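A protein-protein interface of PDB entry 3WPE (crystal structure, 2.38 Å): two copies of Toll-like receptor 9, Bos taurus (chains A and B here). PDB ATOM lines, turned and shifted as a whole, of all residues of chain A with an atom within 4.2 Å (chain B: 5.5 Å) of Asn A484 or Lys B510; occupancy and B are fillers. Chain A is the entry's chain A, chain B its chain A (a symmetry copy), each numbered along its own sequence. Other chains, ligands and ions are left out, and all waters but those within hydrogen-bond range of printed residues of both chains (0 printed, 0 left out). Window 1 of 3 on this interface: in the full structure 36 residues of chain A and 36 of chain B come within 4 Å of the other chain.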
ATOM      1  N   LEU A 457     -15.366  12.628  14.164  1.00  0.00           N
ATOM      2  CA  LEU A 457     -15.467  14.048  13.830  1.00  0.00           C
ATOM      3  C   LEU A 457     -15.961  14.887  15.007  1.00  0.00           C
ATOM      4  O   LEU A 457     -16.329  16.044  14.832  1.00  0.00           O
ATOM      5  CB  LEU A 457     -16.418  14.239  12.645  1.00  0.00           C
ATOM      6  CG  LEU A 457     -15.929  13.737  11.288  1.00  0.00           C
ATOM      7  CD1 LEU A 457     -17.082  13.706  10.302  1.00  0.00           C
ATOM      8  CD2 LEU A 457     -14.805  14.612  10.749  1.00  0.00           C
ATOM      9  N   SER A 458     -15.972  14.330  16.209  1.00  0.00           N
ATOM     10  CA  SER A 458     -16.541  15.062  17.330  1.00  0.00           C
ATOM     11  C   SER A 458     -15.741  16.344  17.605  1.00  0.00           C
ATOM     12  O   SER A 458     -14.570  16.433  17.256  1.00  0.00           O
ATOM     13  CB  SER A 458     -16.602  14.182  18.577  1.00  0.00           C
ATOM     14  OG  SER A 458     -15.313  13.916  19.083  1.00  0.00           O
ATOM     15  N   ASN A 460     -16.189  19.578  16.419  1.00  0.00           N
ATOM     16  CA  ASN A 460     -16.010  20.409  15.245  1.00  0.00           C
ATOM     17  C   ASN A 460     -17.193  21.383  15.192  1.00  0.00           C
ATOM     18  O   ASN A 460     -17.984  21.452  16.137  1.00  0.00           O
ATOM     19  CB  ASN A 460     -15.958  19.519  14.000  1.00  0.00           C
ATOM     20  CG  ASN A 460     -14.568  18.995  13.720  1.00  0.00           C
ATOM     21  OD1 ASN A 460     -13.760  19.672  13.094  1.00  0.00           O
ATOM     22  ND2 ASN A 460     -14.287  17.784  14.164  1.00  0.00           N
ATOM     23  N   ASN A 461     -17.321  22.129  14.101  1.00  0.00           N
ATOM     24  CA  ASN A 461     -18.379  23.133  13.973  1.00  0.00           C
ATOM     25  C   ASN A 461     -19.414  22.782  12.890  1.00  0.00           C
ATOM     26  O   ASN A 461     -19.880  23.652  12.151  1.00  0.00           O
ATOM     27  CB  ASN A 461     -17.749  24.509  13.706  1.00  0.00           C
ATOM     28  CG  ASN A 461     -16.753  24.924  14.794  1.00  0.00           C
ATOM     29  OD1 ASN A 461     -16.853  24.498  15.943  1.00  0.00           O
ATOM     30  ND2 ASN A 461     -15.789  25.763  14.427  1.00  0.00           N
ATOM     31  N   LEU A 462     -19.781  21.504  12.807  1.00  0.00           N
ATOM     32  CA  LEU A 462     -20.802  21.069  11.853  1.00  0.00           C
ATOM     33  C   LEU A 462     -22.167  21.563  12.308  1.00  0.00           C
ATOM     34  O   LEU A 462     -22.542  21.388  13.468  1.00  0.00           O
ATOM     35  CB  LEU A 462     -20.819  19.545  11.704  1.00  0.00           C
ATOM     36  CG  LEU A 462     -19.846  18.920  10.698  1.00  0.00           C
ATOM     37  CD1 LEU A 462     -18.452  19.505  10.811  1.00  0.00           C
ATOM     38  CD2 LEU A 462     -19.794  17.412  10.889  1.00  0.00           C
ATOM     39  N   LEU A 481     -20.038  12.010  15.821  1.00  0.00           N
ATOM     40  CA  LEU A 481     -20.331  13.387  15.442  1.00  0.00           C
ATOM     41  C   LEU A 481     -20.732  14.171  16.678  1.00  0.00           C
ATOM     42  O   LEU A 481     -21.500  15.122  16.607  1.00  0.00           O
ATOM     43  CB  LEU A 481     -21.443  13.425  14.392  1.00  0.00           C
ATOM     44  CG  LEU A 481     -21.020  13.217  12.943  1.00  0.00           C
ATOM     45  CD1 LEU A 481     -22.239  12.913  12.083  1.00  0.00           C
ATOM     46  CD2 LEU A 481     -20.300  14.443  12.418  1.00  0.00           C
ATOM     47  N   SER A 482     -20.164  13.766  17.804  1.00  0.00           N
ATOM     48  CA  SER A 482     -20.435  14.350  19.105  1.00  0.00           C
ATOM     49  C   SER A 482     -19.944  15.804  19.194  1.00  0.00           C
ATOM     50  O   SER A 482     -19.024  16.198  18.487  1.00  0.00           O
ATOM     51  CB  SER A 482     -19.743  13.483  20.166  1.00  0.00           C
ATOM     52  OG  SER A 482     -19.922  13.995  21.469  1.00  0.00           O
ATOM     53  N   HIS A 483     -20.570  16.600  20.057  1.00  0.00           N
ATOM     54  CA  HIS A 483     -20.094  17.957  20.363  1.00  0.00           C
ATOM     55  C   HIS A 483     -19.894  18.808  19.121  1.00  0.00           C
ATOM     56  O   HIS A 483     -18.887  19.502  18.994  1.00  0.00           O
ATOM     57  CB  HIS A 483     -18.789  17.916  21.162  1.00  0.00           C
ATOM     58  CG  HIS A 483     -18.947  17.409  22.563  1.00  0.00           C
ATOM     59  ND1 HIS A 483     -18.629  16.119  22.929  1.00  0.00           N
ATOM     60  CD2 HIS A 483     -19.386  18.022  23.688  1.00  0.00           C
ATOM     61  CE1 HIS A 483     -18.864  15.958  24.220  1.00  0.00           C
ATOM     62  NE2 HIS A 483     -19.326  17.097  24.703  1.00  0.00           N
ATOM     63  N   ASN A 484     -20.845  18.735  18.194  1.00  0.00           N
ATOM     64  CA  ASN A 484     -20.860  19.635  17.046  1.00  0.00           C
ATOM     65  C   ASN A 484     -21.910  20.725  17.291  1.00  0.00           C
ATOM     66  O   ASN A 484     -22.266  20.974  18.438  1.00  0.00           O
ATOM     67  CB  ASN A 484     -21.070  18.848  15.747  1.00  0.00           C
ATOM     68  CG  ASN A 484     -19.767  18.322  15.181  1.00  0.00           C
ATOM     69  OD1 ASN A 484     -18.979  19.072  14.608  1.00  0.00           O
ATOM     70  ND2 ASN A 484     -19.525  17.035  15.353  1.00  0.00           N
ATOM     71  N   SER A 485     -22.380  21.393  16.244  1.00  0.00           N
ATOM     72  CA  SER A 485     -23.355  22.472  16.405  1.00  0.00           C
ATOM     73  C   SER A 485     -24.611  22.138  15.624  1.00  0.00           C
ATOM     74  O   SER A 485     -25.282  23.026  15.103  1.00  0.00           O
ATOM     75  CB  SER A 485     -22.765  23.787  15.881  1.00  0.00           C
ATOM     76  OG  SER A 485     -21.474  24.038  16.409  1.00  0.00           O
ATOM     77  N   ILE A 486     -24.933  20.850  15.551  1.00  0.00           N
ATOM     78  CA  ILE A 486     -25.889  20.365  14.560  1.00  0.00           C
ATOM     79  C   ILE A 486     -27.313  20.690  14.985  1.00  0.00           C
ATOM     80  O   ILE A 486     -27.794  20.171  15.987  1.00  0.00           O
ATOM     81  CB  ILE A 486     -25.725  18.850  14.302  1.00  0.00           C
ATOM     82  CG1 ILE A 486     -24.285  18.546  13.865  1.00  0.00           C
ATOM     83  CG2 ILE A 486     -26.686  18.383  13.214  1.00  0.00           C
ATOM     84  CD1 ILE A 486     -23.943  17.073  13.808  1.00  0.00           C
ATOM     85  N   HIS A 508     -24.483  15.629  22.424  1.00  0.00           N
ATOM     86  CA  HIS A 508     -24.031  17.029  22.547  1.00  0.00           C
ATOM     87  C   HIS A 508     -24.227  17.798  21.245  1.00  0.00           C
ATOM     88  O   HIS A 508     -23.271  18.250  20.614  1.00  0.00           O
ATOM     89  CB  HIS A 508     -22.580  17.110  23.053  1.00  0.00           C
ATOM     90  CG  HIS A 508     -22.418  16.670  24.479  1.00  0.00           C
ATOM     91  ND1 HIS A 508     -21.867  15.457  24.827  1.00  0.00           N
ATOM     92  CD2 HIS A 508     -22.754  17.272  25.644  1.00  0.00           C
ATOM     93  CE1 HIS A 508     -21.859  15.333  26.144  1.00  0.00           C
ATOM     94  NE2 HIS A 508     -22.400  16.418  26.662  1.00  0.00           N
ATOM     95  N   ASN A 509     -25.489  17.921  20.838  1.00  0.00           N
ATOM     96  CA  ASN A 509     -25.848  18.665  19.637  1.00  0.00           C
ATOM     97  C   ASN A 509     -27.215  19.314  19.837  1.00  0.00           C
ATOM     98  O   ASN A 509     -27.752  19.268  20.929  1.00  0.00           O
ATOM     99  CB  ASN A 509     -25.836  17.740  18.418  1.00  0.00           C
ATOM    100  CG  ASN A 509     -24.452  17.597  17.806  1.00  0.00           C
ATOM    101  OD1 ASN A 509     -23.913  18.543  17.232  1.00  0.00           O
ATOM    102  ND2 ASN A 509     -23.883  16.404  17.899  1.00  0.00           N
ATOM    103  N   SER B 485     -24.200  28.532  18.920  1.00  0.00           N
ATOM    104  CA  SER B 485     -23.213  27.601  18.371  1.00  0.00           C
ATOM    105  C   SER B 485     -21.925  28.346  18.080  1.00  0.00           C
ATOM    106  O   SER B 485     -21.210  28.018  17.136  1.00  0.00           O
ATOM    107  CB  SER B 485     -23.748  26.983  17.074  1.00  0.00           C
ATOM    108  OG  SER B 485     -25.060  26.470  17.231  1.00  0.00           O
ATOM    109  N   ILE B 486     -21.626  29.348  18.902  1.00  0.00           N
ATOM    110  CA  ILE B 486     -20.629  30.350  18.539  1.00  0.00           C
ATOM    111  C   ILE B 486     -19.223  29.796  18.714  1.00  0.00           C
ATOM    112  O   ILE B 486     -18.806  29.504  19.830  1.00  0.00           O
ATOM    113  CB  ILE B 486     -20.809  31.653  19.349  1.00  0.00           C
ATOM    114  CG1 ILE B 486     -22.230  32.200  19.151  1.00  0.00           C
ATOM    115  CG2 ILE B 486     -19.802  32.708  18.903  1.00  0.00           C
ATOM    116  CD1 ILE B 486     -22.599  33.342  20.073  1.00  0.00           C
ATOM    117  N   SER B 487     -18.513  29.664  17.592  1.00  0.00           N
ATOM    118  CA  SER B 487     -17.168  29.095  17.538  1.00  0.00           C
ATOM    119  C   SER B 487     -16.128  30.136  17.107  1.00  0.00           C
ATOM    120  O   SER B 487     -15.013  29.797  16.745  1.00  0.00           O
ATOM    121  CB  SER B 487     -17.148  27.951  16.535  1.00  0.00           C
ATOM    122  OG  SER B 487     -17.457  28.445  15.239  1.00  0.00           O
ATOM    123  N   GLN B 488     -16.507  31.403  17.154  1.00  0.00           N
ATOM    124  CA  GLN B 488     -15.680  32.492  16.650  1.00  0.00           C
ATOM    125  C   GLN B 488     -14.451  32.743  17.534  1.00  0.00           C
ATOM    126  O   GLN B 488     -14.471  32.480  18.737  1.00  0.00           O
ATOM    127  CB  GLN B 488     -16.540  33.751  16.588  1.00  0.00           C
ATOM    128  CG  GLN B 488     -15.958  34.920  15.828  1.00  0.00           C
ATOM    129  CD  GLN B 488     -17.011  35.978  15.558  1.00  0.00           C
ATOM    130  OE1 GLN B 488     -18.038  36.027  16.235  1.00  0.00           O
ATOM    131  NE2 GLN B 488     -16.770  36.822  14.561  1.00  0.00           N
ATOM    132  N   HIS B 508     -22.543  28.661  27.468  1.00  0.00           N
ATOM    133  CA  HIS B 508     -22.973  27.545  26.602  1.00  0.00           C
ATOM    134  C   HIS B 508     -22.693  27.838  25.132  1.00  0.00           C
ATOM    135  O   HIS B 508     -23.605  27.941  24.312  1.00  0.00           O
ATOM    136  CB  HIS B 508     -24.447  27.177  26.848  1.00  0.00           C
ATOM    137  CG  HIS B 508     -24.693  26.557  28.192  1.00  0.00           C
ATOM    138  ND1 HIS B 508     -25.285  27.239  29.231  1.00  0.00           N
ATOM    139  CD2 HIS B 508     -24.407  25.325  28.674  1.00  0.00           C
ATOM    140  CE1 HIS B 508     -25.366  26.454  30.292  1.00  0.00           C
ATOM    141  NE2 HIS B 508     -24.831  25.289  29.982  1.00  0.00           N
ATOM    142  N   ASN B 509     -21.409  27.992  24.814  1.00  0.00           N
ATOM    143  CA  ASN B 509     -20.972  28.231  23.444  1.00  0.00           C
ATOM    144  C   ASN B 509     -19.605  27.587  23.233  1.00  0.00           C
ATOM    145  O   ASN B 509     -19.127  26.881  24.103  1.00  0.00           O
ATOM    146  CB  ASN B 509     -20.938  29.733  23.154  1.00  0.00           C
ATOM    147  CG  ASN B 509     -22.291  30.276  22.722  1.00  0.00           C
ATOM    148  OD1 ASN B 509     -22.779  29.965  21.636  1.00  0.00           O
ATOM    149  ND2 ASN B 509     -22.888  31.114  23.557  1.00  0.00           N
ATOM    150  N   LYS B 510     -18.993  27.794  22.075  1.00  0.00           N
ATOM    151  CA  LYS B 510     -17.658  27.254  21.812  1.00  0.00           C
ATOM    152  C   LYS B 510     -16.652  28.385  21.582  1.00  0.00           C
ATOM    153  O   LYS B 510     -15.784  28.261  20.728  1.00  0.00           O
ATOM    154  CB  LYS B 510     -17.666  26.343  20.573  1.00  0.00           C
ATOM    155  CG  LYS B 510     -18.683  25.215  20.571  1.00  0.00           C
ATOM    156  CD  LYS B 510     -18.548  24.423  19.276  1.00  0.00           C
ATOM    157  CE  LYS B 510     -19.763  23.564  18.972  1.00  0.00           C
ATOM    158  NZ  LYS B 510     -19.884  22.396  19.888  1.00  0.00           N
ATOM    159  N   LEU B 511     -16.761  29.476  22.336  1.00  0.00           N
ATOM    160  CA  LEU B 511     -15.882  30.630  22.121  1.00  0.00           C
ATOM    161  C   LEU B 511     -14.411  30.268  22.315  1.00  0.00           C
ATOM    162  O   LEU B 511     -14.023  29.766  23.364  1.00  0.00           O
ATOM    163  CB  LEU B 511     -16.234  31.773  23.072  1.00  0.00           C
ATOM    164  CG  LEU B 511     -17.644  32.358  22.998  1.00  0.00           C
ATOM    165  CD1 LEU B 511     -17.726  33.625  23.829  1.00  0.00           C
ATOM    166  CD2 LEU B 511     -18.047  32.663  21.570  1.00  0.00           C
ATOM    167  N   ASP B 512     -13.593  30.517  21.301  1.00  0.00           N
ATOM    168  CA  ASP B 512     -12.159  30.322  21.449  1.00  0.00           C
ATOM    169  C   ASP B 512     -11.490  31.632  21.851  1.00  0.00           C
ATOM    170  O   ASP B 512     -11.518  32.627  21.109  1.00  0.00           O
ATOM    171  CB  ASP B 512     -11.525  29.745  20.183  1.00  0.00           C
ATOM    172  CG  ASP B 512     -10.309  28.897  20.495  1.00  0.00           C
ATOM    173  OD1 ASP B 512      -9.662  29.151  21.538  1.00  0.00           O
ATOM    174  OD2 ASP B 512     -10.009  27.973  19.713  1.00  0.00           O
ATOM    175  N   ASN B 533     -18.164  26.944  28.142  1.00  0.00           N
ATOM    176  CA  ASN B 533     -17.436  26.992  26.886  1.00  0.00           C
ATOM    177  C   ASN B 533     -16.234  26.063  26.986  1.00  0.00           C
ATOM    178  O   ASN B 533     -15.129  26.405  26.587  1.00  0.00           O
ATOM    179  CB  ASN B 533     -16.983  28.418  26.576  1.00  0.00           C
ATOM    180  CG  ASN B 533     -18.097  29.288  26.046  1.00  0.00           C
ATOM    181  OD1 ASN B 533     -18.142  29.582  24.857  1.00  0.00           O
ATOM    182  ND2 ASN B 533     -18.988  29.720  26.924  1.00  0.00           N
ATOM    183  N   GLN B 535     -15.384  23.250  25.515  1.00  0.00           N
ATOM    184  CA  GLN B 535     -14.849  22.564  24.346  1.00  0.00           C
ATOM    185  C   GLN B 535     -13.509  23.185  23.901  1.00  0.00           C
ATOM    186  O   GLN B 535     -12.540  22.453  23.722  1.00  0.00           O
ATOM    187  CB  GLN B 535     -15.898  22.501  23.221  1.00  0.00           C
ATOM    188  CG  GLN B 535     -15.464  21.764  21.957  1.00  0.00           C
ATOM    189  CD  GLN B 535     -16.602  21.593  20.939  1.00  0.00           C
ATOM    190  OE1 GLN B 535     -17.768  21.398  21.305  1.00  0.00           O
ATOM    191  NE2 GLN B 535     -16.265  21.669  19.656  1.00  0.00           N
ATOM    192  N   PRO B 536     -13.438  24.524  23.736  1.00  0.00           N
ATOM    193  CA  PRO B 536     -12.118  25.151  23.500  1.00  0.00           C
ATOM    194  C   PRO B 536     -11.112  24.942  24.631  1.00  0.00           C
ATOM    195  O   PRO B 536      -9.994  24.523  24.375  1.00  0.00           O
ATOM    196  CB  PRO B 536     -12.445  26.640  23.356  1.00  0.00           C
ATOM    197  CG  PRO B 536     -13.866  26.672  22.919  1.00  0.00           C
ATOM    198  CD  PRO B 536     -14.540  25.471  23.499  1.00  0.00           C
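The backbone carbonyl oxygen (O) of Asn A484 is in hydrogen-bond range of the side-chain amino group (NZ) of Lys B510, at 3.1 Å. The backbone carbonyl oxygen (O) of His A483 sits close to the side-chain amide oxygen (OE1) of Gln B535 (3.2 Å). The backbone carbonyl oxygen (O) of His A483 lies within hydrogen-bond range of the side-chain amino group (NZ) of Lys B510, at 3.2 Å. The side-chain amide nitrogen (ND2) of Asn A461 sits at hydrogen-bond distance from the side-chain hydroxyl (OG) of Ser B487 (3.3 Å).
A ring nitrogen (NE2) of His A483 is in hydrogen-bond range of a ring nitrogen (ND1) of His A508, at 3.0 Å. The side-chain amide nitrogen (ND2) of Asn A484 is in hydrogen-bond range of the backbone carbonyl oxygen (O) of Leu A481, at 3.0 Å. The backbone NH of Leu A462 lies within hydrogen-bond range of the side-chain amide oxygen of Asn A484. The backbone carbonyl oxygen (O) of Ile B486 lies within hydrogen-bond range of the backbone NH (N) of Lys B510 (2.8 Å). The backbone carbonyl oxygen of Ser A482 is in hydrogen-bond range of the side-chain amide nitrogen of Asn A484. The side-chain amide oxygen of Asn B533 sits at hydrogen-bond distance from the backbone NH of Lys B510 (3.4 Å).
Among the printed residues, pairs that only touch across the chains: Asn A460 with Lys B510 (3.96 Å), Asn A460 with Gln B535 (3.9 Å), Asn A461 with Lys B510 (3.7 Å), Ser A485 with Ser B485 (3.6 Å) and Ser A485 with Lys B510 (3.1 Å).
Printed residues of chain B within 4 Å of Asn A461: Ser B487 and Lys B510. Of the printed residues of chain B, Asn A484 touches Lys B510 (3.1 Å). Asn B509 touches none of the printed residues of chain A. Of chain A, only Asn A460 (3.96 Å), Asn A461 (3.7 Å), His A483 (3.2 Å), Asn A484 (3.1 Å) and Ser A485 (3.1 Å) come within 4 Å of Lys B510. Printed residues of chain A within 4 Å of Gln B535: Asn A460 (3.9 Å) and His A483 (3.2 Å). The nearest printed residue of chain A that does not touch Lys B510 is His A508 (5.4 Å).
Of the 12 printed residues of chain B, 4 touch a printed residue of chain A. Of the 13 printed residues of chain A, 5 touch a printed residue of chain B. Hydrophobic or aromatic side chains of chain A within 4 Å of the printed part of chain B: His A483. Among the printed residues, no Asp or Glu carboxylate lies within 4 Å of a Lys or Arg side-chain nitrogen of the other chain.
Ser A485 touches its own counterpart, Ser B485. Positions printed for both chains: 485, 486, 508 and 509. Of the 9 pairs that touch across the chains among the printed residues, 1 has its exchanged pair printed and touching as well.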
